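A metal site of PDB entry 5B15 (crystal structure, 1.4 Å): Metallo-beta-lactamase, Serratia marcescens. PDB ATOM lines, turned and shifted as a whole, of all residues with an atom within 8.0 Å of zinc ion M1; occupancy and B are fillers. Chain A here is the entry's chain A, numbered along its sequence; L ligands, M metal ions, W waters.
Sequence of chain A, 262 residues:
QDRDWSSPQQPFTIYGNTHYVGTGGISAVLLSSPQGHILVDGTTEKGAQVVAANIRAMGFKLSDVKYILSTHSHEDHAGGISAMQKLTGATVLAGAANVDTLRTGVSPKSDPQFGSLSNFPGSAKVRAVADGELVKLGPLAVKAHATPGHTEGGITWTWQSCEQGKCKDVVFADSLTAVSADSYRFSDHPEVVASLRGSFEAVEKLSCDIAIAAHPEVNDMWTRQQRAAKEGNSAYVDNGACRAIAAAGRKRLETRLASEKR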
ATOM      1  N   TRP A   5      -2.311 -20.715  15.642  1.00  0.00           N
ATOM      2  CA  TRP A   5      -2.826 -19.463  15.120  1.00  0.00           C
ATOM      3  C   TRP A   5      -2.662 -19.296  13.639  1.00  0.00           C
ATOM      4  O   TRP A   5      -3.450 -18.593  13.007  1.00  0.00           O
ATOM      5  CB  TRP A   5      -2.157 -18.270  15.755  1.00  0.00           C
ATOM      6  CG  TRP A   5      -2.387 -18.034  17.199  1.00  0.00           C
ATOM      7  CD1 TRP A   5      -3.299 -18.644  18.004  1.00  0.00           C
ATOM      8  CD2 TRP A   5      -1.673 -17.101  18.005  1.00  0.00           C
ATOM      9  NE1 TRP A   5      -3.187 -18.125  19.285  1.00  0.00           N
ATOM     10  CE2 TRP A   5      -2.197 -17.190  19.300  1.00  0.00           C
ATOM     11  CE3 TRP A   5      -0.626 -16.201  17.744  1.00  0.00           C
ATOM     12  CZ2 TRP A   5      -1.715 -16.383  20.343  1.00  0.00           C
ATOM     13  CZ3 TRP A   5      -0.139 -15.417  18.792  1.00  0.00           C
ATOM     14  CH2 TRP A   5      -0.666 -15.543  20.067  1.00  0.00           C
ATOM     15  N   THR A  71     -11.840  -6.953  15.022  1.00  0.00           N
ATOM     16  CA  THR A  71     -12.352  -7.123  16.380  1.00  0.00           C
ATOM     17  C   THR A  71     -11.466  -6.359  17.341  1.00  0.00           C
ATOM     18  O   THR A  71     -11.893  -5.376  17.989  1.00  0.00           O
ATOM     19  CB  THR A  71     -12.443  -8.617  16.768  1.00  0.00           C
ATOM     20  OG1 THR A  71     -11.187  -9.247  16.567  1.00  0.00           O
ATOM     21  CG2 THR A  71     -13.565  -9.317  16.030  1.00  0.00           C
ATOM     22  N   HIS A  72     -10.227  -6.808  17.474  1.00  0.00           N
ATOM     23  CA  HIS A  72      -9.281  -6.044  18.303  1.00  0.00           C
ATOM     24  C   HIS A  72      -7.849  -6.248  17.869  1.00  0.00           C
ATOM     25  O   HIS A  72      -7.497  -7.164  17.113  1.00  0.00           O
ATOM     26  CB  HIS A  72      -9.507  -6.370  19.795  1.00  0.00           C
ATOM     27  CG  HIS A  72      -8.949  -7.681  20.237  1.00  0.00           C
ATOM     28  ND1 HIS A  72      -9.697  -8.831  20.257  1.00  0.00           N
ATOM     29  CD2 HIS A  72      -7.696  -8.042  20.605  1.00  0.00           C
ATOM     30  CE1 HIS A  72      -8.959  -9.830  20.703  1.00  0.00           C
ATOM     31  NE2 HIS A  72      -7.732  -9.378  20.940  1.00  0.00           N
ATOM     32  N   SER A  73      -7.001  -5.377  18.406  1.00  0.00           N
ATOM     33  CA  SER A  73      -5.666  -5.092  17.861  1.00  0.00           C
ATOM     34  C   SER A  73      -4.578  -5.847  18.603  1.00  0.00           C
ATOM     35  O   SER A  73      -3.686  -5.247  19.204  1.00  0.00           O
ATOM     36  CB  SER A  73      -5.455  -3.603  17.861  1.00  0.00           C
ATOM     37  OG  SER A  73      -5.766  -3.040  19.126  1.00  0.00           O
ATOM     38  N   HIS A  74      -4.646  -7.190  18.599  1.00  0.00           N
ATOM     39  CA  HIS A  74      -3.534  -8.045  19.042  1.00  0.00           C
ATOM     40  C   HIS A  74      -3.051  -8.891  17.867  1.00  0.00           C
ATOM     41  O   HIS A  74      -3.805  -9.126  16.905  1.00  0.00           O
ATOM     42  CB  HIS A  74      -3.988  -8.979  20.180  1.00  0.00           C
ATOM     43  CG  HIS A  74      -4.255  -8.265  21.466  1.00  0.00           C
ATOM     44  ND1 HIS A  74      -5.100  -8.769  22.417  1.00  0.00           N
ATOM     45  CD2 HIS A  74      -3.786  -7.092  21.957  1.00  0.00           C
ATOM     46  CE1 HIS A  74      -5.122  -7.961  23.464  1.00  0.00           C
ATOM     47  NE2 HIS A  74      -4.335  -6.935  23.208  1.00  0.00           N
ATOM     48  N   GLU A  75      -1.829  -9.395  17.989  1.00  0.00           N
ATOM     49  CA  GLU A  75      -1.158 -10.066  16.895  1.00  0.00           C
ATOM     50  C   GLU A  75      -1.911 -11.261  16.376  1.00  0.00           C
ATOM     51  O   GLU A  75      -1.835 -11.563  15.162  1.00  0.00           O
ATOM     52  CB  GLU A  75       0.242 -10.537  17.308  1.00  0.00           C
ATOM     53  CG  GLU A  75       0.292 -11.713  18.281  1.00  0.00           C
ATOM     54  CD  GLU A  75       1.702 -12.198  18.599  1.00  0.00           C
ATOM     55  OE1 GLU A  75       1.940 -12.543  19.777  1.00  0.00           O
ATOM     56  OE2 GLU A  75       2.494 -12.368  17.657  1.00  0.00           O
ATOM     57  N   ASP A  76      -2.650 -11.966  17.228  1.00  0.00           N
ATOM     58  CA  ASP A  76      -3.350 -13.178  16.793  1.00  0.00           C
ATOM     59  C   ASP A  76      -4.563 -12.932  15.893  1.00  0.00           C
ATOM     60  O   ASP A  76      -4.841 -13.769  15.030  1.00  0.00           O
ATOM     61  CB  ASP A  76      -3.689 -14.126  17.953  1.00  0.00           C
ATOM     62  CG  ASP A  76      -4.411 -13.460  19.121  1.00  0.00           C
ATOM     63  OD1 ASP A  76      -4.254 -12.215  19.410  1.00  0.00           O
ATOM     64  OD2 ASP A  76      -5.098 -14.265  19.827  1.00  0.00           O
ATOM     65  N   HIS A  77      -5.234 -11.797  16.075  1.00  0.00           N
ATOM     66  CA  HIS A  77      -6.416 -11.453  15.256  1.00  0.00           C
ATOM     67  C   HIS A  77      -6.101 -10.444  14.165  1.00  0.00           C
ATOM     68  O   HIS A  77      -6.765 -10.436  13.108  1.00  0.00           O
ATOM     69  CB  HIS A  77      -7.522 -10.910  16.170  1.00  0.00           C
ATOM     70  CG  HIS A  77      -7.786 -11.782  17.338  1.00  0.00           C
ATOM     71  ND1 HIS A  77      -8.523 -12.956  17.225  1.00  0.00           N
ATOM     72  CD2 HIS A  77      -7.279 -11.762  18.589  1.00  0.00           C
ATOM     73  CE1 HIS A  77      -8.454 -13.608  18.391  1.00  0.00           C
ATOM     74  NE2 HIS A  77      -7.694 -12.912  19.224  1.00  0.00           N
ATOM     75  N   ALA A  78      -5.171  -9.525  14.450  1.00  0.00           N
ATOM     76  CA  ALA A  78      -4.885  -8.366  13.610  1.00  0.00           C
ATOM     77  C   ALA A  78      -3.545  -8.462  12.913  1.00  0.00           C
ATOM     78  O   ALA A  78      -3.268  -7.601  12.066  1.00  0.00           O
ATOM     79  CB  ALA A  78      -4.903  -7.073  14.427  1.00  0.00           C
ATOM     80  N   SER A 107       0.681  -2.300  20.915  1.00  0.00           N
ATOM     81  CA  SER A 107      -0.421  -2.079  21.870  1.00  0.00           C
ATOM     82  C   SER A 107       0.081  -1.127  22.981  1.00  0.00           C
ATOM     83  O   SER A 107       1.250  -1.174  23.350  1.00  0.00           O
ATOM     84  CB  SER A 107      -0.916  -3.399  22.490  1.00  0.00           C
ATOM     85  OG  SER A 107      -1.651  -4.194  21.538  1.00  0.00           O
ATOM     86  N   ASP A 111      -3.308  -1.428  27.903  1.00  0.00           N
ATOM     87  CA  ASP A 111      -3.708  -2.841  27.686  1.00  0.00           C
ATOM     88  C   ASP A 111      -3.269  -3.691  28.869  1.00  0.00           C
ATOM     89  O   ASP A 111      -2.109  -3.708  29.197  1.00  0.00           O
ATOM     90  CB  ASP A 111      -3.070  -3.331  26.376  1.00  0.00           C
ATOM     91  CG  ASP A 111      -3.627  -4.685  25.900  1.00  0.00           C
ATOM     92  OD1 ASP A 111      -3.615  -5.663  26.658  1.00  0.00           O
ATOM     93  OD2 ASP A 111      -4.016  -4.731  24.756  1.00  0.00           O
ATOM     94  N   GLN A 113      -2.459  -6.690  29.033  1.00  0.00           N
ATOM     95  CA  GLN A 113      -1.369  -7.540  28.654  1.00  0.00           C
ATOM     96  C   GLN A 113      -0.084  -6.774  28.284  1.00  0.00           C
ATOM     97  O   GLN A 113       0.885  -7.410  27.905  1.00  0.00           O
ATOM     98  CB  GLN A 113      -1.788  -8.499  27.542  1.00  0.00           C
ATOM     99  CG  GLN A 113      -2.893  -9.465  27.929  1.00  0.00           C
ATOM    100  CD  GLN A 113      -3.152 -10.458  26.824  1.00  0.00           C
ATOM    101  OE1 GLN A 113      -2.400 -11.436  26.686  1.00  0.00           O
ATOM    102  NE2 GLN A 113      -4.169 -10.208  26.011  1.00  0.00           N
ATOM    103  N   LEU A 117       2.823  -8.606  25.308  1.00  0.00           N
ATOM    104  CA  LEU A 117       2.337  -8.732  23.930  1.00  0.00           C
ATOM    105  C   LEU A 117       3.497  -8.634  22.936  1.00  0.00           C
ATOM    106  O   LEU A 117       4.464  -7.910  23.192  1.00  0.00           O
ATOM    107  CB  LEU A 117       1.330  -7.627  23.634  1.00  0.00           C
ATOM    108  CG  LEU A 117       0.015  -7.707  24.441  1.00  0.00           C
ATOM    109  CD1 LEU A 117      -0.758  -6.396  24.383  1.00  0.00           C
ATOM    110  CD2 LEU A 117      -0.831  -8.808  23.853  1.00  0.00           C
ATOM    111  N   HIS A 150     -11.098  -6.280  26.906  1.00  0.00           N
ATOM    112  CA  HIS A 150      -9.888  -6.973  26.490  1.00  0.00           C
ATOM    113  C   HIS A 150      -8.938  -5.990  25.751  1.00  0.00           C
ATOM    114  O   HIS A 150      -7.719  -6.066  25.917  1.00  0.00           O
ATOM    115  CB  HIS A 150     -10.296  -8.206  25.671  1.00  0.00           C
ATOM    116  CG  HIS A 150      -9.163  -9.045  25.168  1.00  0.00           C
ATOM    117  ND1 HIS A 150      -8.549 -10.042  25.910  1.00  0.00           N
ATOM    118  CD2 HIS A 150      -8.548  -9.070  23.964  1.00  0.00           C
ATOM    119  CE1 HIS A 150      -7.642 -10.657  25.162  1.00  0.00           C
ATOM    120  NE2 HIS A 150      -7.586 -10.051  24.003  1.00  0.00           N
ATOM    121  N   THR A 151      -9.524  -5.044  25.004  1.00  0.00           N
ATOM    122  CA  THR A 151      -8.813  -3.856  24.495  1.00  0.00           C
ATOM    123  C   THR A 151      -9.840  -2.728  24.577  1.00  0.00           C
ATOM    124  O   THR A 151     -11.062  -2.942  24.590  1.00  0.00           O
ATOM    125  CB  THR A 151      -8.361  -4.004  23.040  1.00  0.00           C
ATOM    126  OG1 THR A 151      -9.493  -4.100  22.168  1.00  0.00           O
ATOM    127  CG2 THR A 151      -7.370  -5.150  22.843  1.00  0.00           C
ATOM    128  N   ASP A 174     -16.106 -10.493  19.459  1.00  0.00           N
ATOM    129  CA  ASP A 174     -14.793 -10.146  19.975  1.00  0.00           C
ATOM    130  C   ASP A 174     -14.530 -10.872  21.277  1.00  0.00           C
ATOM    131  O   ASP A 174     -15.438 -11.366  21.930  1.00  0.00           O
ATOM    132  CB  ASP A 174     -14.709  -8.629  20.214  1.00  0.00           C
ATOM    133  CG  ASP A 174     -13.290  -8.121  20.380  1.00  0.00           C
ATOM    134  OD1 ASP A 174     -12.341  -8.823  20.048  1.00  0.00           O
ATOM    135  OD2 ASP A 174     -13.186  -6.981  20.938  1.00  0.00           O
ATOM    136  N   SER A 175     -13.233 -10.992  21.587  1.00  0.00           N
ATOM    137  CA  SER A 175     -12.838 -11.533  22.880  1.00  0.00           C
ATOM    138  C   SER A 175     -13.291 -10.645  24.042  1.00  0.00           C
ATOM    139  O   SER A 175     -13.132  -9.437  23.993  1.00  0.00           O
ATOM    140  CB  SER A 175     -11.332 -11.715  22.871  1.00  0.00           C
ATOM    141  OG  SER A 175     -10.979 -12.545  21.770  1.00  0.00           O
ATOM    142  N   LEU A 176     -13.788 -11.293  25.101  1.00  0.00           N
ATOM    143  CA  LEU A 176     -14.262 -10.645  26.325  1.00  0.00           C
ATOM    144  C   LEU A 176     -13.432 -11.040  27.538  1.00  0.00           C
ATOM    145  O   LEU A 176     -13.929 -11.057  28.642  1.00  0.00           O
ATOM    146  CB  LEU A 176     -15.727 -11.042  26.548  1.00  0.00           C
ATOM    147  CG  LEU A 176     -16.687 -10.712  25.415  1.00  0.00           C
ATOM    148  CD1 LEU A 176     -18.102 -11.126  25.708  1.00  0.00           C
ATOM    149  CD2 LEU A 176     -16.611  -9.267  24.965  1.00  0.00           C
ATOM    150  N   THR A 177     -12.195 -11.476  27.298  1.00  0.00           N
ATOM    151  CA  THR A 177     -11.391 -12.115  28.322  1.00  0.00           C
ATOM    152  C   THR A 177     -10.480 -11.183  29.114  1.00  0.00           C
ATOM    153  O   THR A 177      -9.712 -10.407  28.551  1.00  0.00           O
ATOM    154  CB  THR A 177     -10.506 -13.209  27.699  1.00  0.00           C
ATOM    155  OG1 THR A 177      -9.645 -12.623  26.716  1.00  0.00           O
ATOM    156  CG2 THR A 177     -11.363 -14.286  27.077  1.00  0.00           C
ATOM    157  N   VAL A 179      -7.380 -11.038  30.792  1.00  0.00           N
ATOM    158  CA  VAL A 179      -6.053 -11.622  30.858  1.00  0.00           C
ATOM    159  C   VAL A 179      -5.055 -10.529  31.023  1.00  0.00           C
ATOM    160  O   VAL A 179      -5.210  -9.453  30.485  1.00  0.00           O
ATOM    161  CB  VAL A 179      -5.740 -12.434  29.621  1.00  0.00           C
ATOM    162  CG1 VAL A 179      -6.518 -13.709  29.602  1.00  0.00           C
ATOM    163  CG2 VAL A 179      -6.027 -11.707  28.359  1.00  0.00           C
ATOM    164  N   ALA A 214     -13.933 -14.982  17.999  1.00  0.00           N
ATOM    165  CA  ALA A 214     -12.612 -14.672  17.464  1.00  0.00           C
ATOM    166  C   ALA A 214     -11.638 -15.848  17.622  1.00  0.00           C
ATOM    167  O   ALA A 214     -10.874 -16.184  16.714  1.00  0.00           O
ATOM    168  CB  ALA A 214     -12.075 -13.406  18.130  1.00  0.00           C
ATOM    169  N   HIS A 215     -11.649 -16.463  18.817  1.00  0.00           N
ATOM    170  CA  HIS A 215     -11.056 -17.810  18.980  1.00  0.00           C
ATOM    171  C   HIS A 215     -12.163 -18.831  18.806  1.00  0.00           C
ATOM    172  O   HIS A 215     -13.102 -18.865  19.587  1.00  0.00           O
ATOM    173  CB  HIS A 215     -10.427 -17.947  20.381  1.00  0.00           C
ATOM    174  CG  HIS A 215      -9.185 -17.159  20.552  1.00  0.00           C
ATOM    175  ND1 HIS A 215      -7.930 -17.640  20.243  1.00  0.00           N
ATOM    176  CD2 HIS A 215      -9.011 -15.863  20.917  1.00  0.00           C
ATOM    177  CE1 HIS A 215      -7.040 -16.679  20.413  1.00  0.00           C
ATOM    178  NE2 HIS A 215      -7.667 -15.584  20.781  1.00  0.00           N
HETATM  179  O1  LIG L   1      -1.362 -14.891  23.932  1.00  0.00           O
HETATM  180  C1  LIG L   1      -2.458 -15.369  23.707  1.00  0.00           C
HETATM  181  O2  LIG L   1      -2.596 -16.667  23.658  1.00  0.00           O
HETATM  182  C2  LIG L   1      -3.623 -14.508  23.252  1.00  0.00           C
HETATM  183  C3  LIG L   1      -3.370 -13.053  23.704  1.00  0.00           C
HETATM  184  C4  LIG L   1      -2.505 -12.316  22.686  1.00  0.00           C
HETATM  185  O3  LIG L   1      -4.585 -12.301  23.941  1.00  0.00           O
HETATM  186  C5  LIG L   1      -4.927 -15.203  23.646  1.00  0.00           C
HETATM  187  C6  LIG L   1      -5.293 -15.493  25.121  1.00  0.00           C
HETATM  188  C7  LIG L   1      -4.388 -14.833  26.165  1.00  0.00           C
HETATM  189  N1  LIG L   1      -6.065 -14.448  23.093  1.00  0.00           N
HETATM  190  C8  LIG L   1      -7.008 -14.412  23.926  1.00  0.00           C
HETATM  191  C9  LIG L   1      -8.286 -13.802  23.570  1.00  0.00           C
HETATM  192  O4  LIG L   1      -8.376 -13.142  22.452  1.00  0.00           O
HETATM  193  O5  LIG L   1      -9.262 -13.929  24.345  1.00  0.00           O
HETATM  194  C10 LIG L   1      -6.764 -15.043  25.275  1.00  0.00           C
HETATM  195  S1  LIG L   1      -7.932 -16.341  25.744  1.00  0.00           S
HETATM  196  C11 LIG L   1      -8.130 -17.336  24.284  1.00  0.00           C
HETATM  197  C12 LIG L   1      -9.375 -18.187  24.480  1.00  0.00           C
HETATM  198  N2  LIG L   1      -8.935 -19.581  24.340  1.00  0.00           N
HETATM  199  C13 LIG L   1      -7.722 -19.578  23.494  1.00  0.00           C
HETATM  200  C14 LIG L   1      -6.993 -18.287  23.910  1.00  0.00           C
HETATM  201  C15 LIG L   1      -6.966 -20.893  23.699  1.00  0.00           C
HETATM  202  N3  LIG L   1      -7.529 -21.757  24.770  1.00  0.00           N
HETATM  203  S2  LIG L   1      -8.743 -22.818  24.415  1.00  0.00           S
HETATM  204  O6  LIG L   1      -8.909 -23.824  25.449  1.00  0.00           O
HETATM  205  O7  LIG L   1      -9.972 -22.069  24.180  1.00  0.00           O
HETATM  206  N4  LIG L   1      -8.300 -23.702  23.132  1.00  0.00           N
HETATM  207 ZN    ZN M   1      -6.454 -10.304  22.222  1.00  0.00          ZN
HETATM  208 ZN    ZN M   2      -6.760 -13.667  21.014  1.00  0.00          ZN
HETATM  209  O   HOH W   1      -5.829 -11.928  21.646  1.00  0.00           O
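Water W1 is bound to zinc ion M1, at 1.8 Å.
NE2 of His 72 binds zinc ion M1, 2.0 Å away.
ND1 of His 74 binds zinc ion M1 (2.1 Å).
Zinc ion M1 is bound by NE2 of His 150 (2.1 Å).
Zinc ion M1 has four donor atoms within binding distance.
ND1 of His 150 is in hydrogen-bond range of O of Thr 177 (2.9 Å).
A ring nitrogen (NE2) of His 74 sits at hydrogen-bond distance from the side-chain carboxylate of Asp 111.
A ring nitrogen (ND1) of His 72 is in hydrogen-bond range of the side-chain carboxylate (OD1) of Asp 174, at 2.7 Å.
The side-chain amide nitrogen (NE2) of Gln 113 lies within hydrogen-bond range of an oxygen (O3) of the ligand (3.0 Å).
An oxygen (O5) of the ligand is in hydrogen-bond range of the side-chain hydroxyl (OG1) of Thr 177 (2.7 Å).
OG of Ser 175 lies close to O5 of the ligand (3.4 Å).
Water W1 lies within hydrogen-bond range of an oxygen (O3) of the ligand (2.6 Å) and the side-chain carboxylate (OD1) of Asp 76 (2.8 Å).
Of the 22 residues printed, 3 come within 4 Å of zinc ion M1.
The nearest printed residue that does not touch zinc ion M1 is His 77 (4.001 Å).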
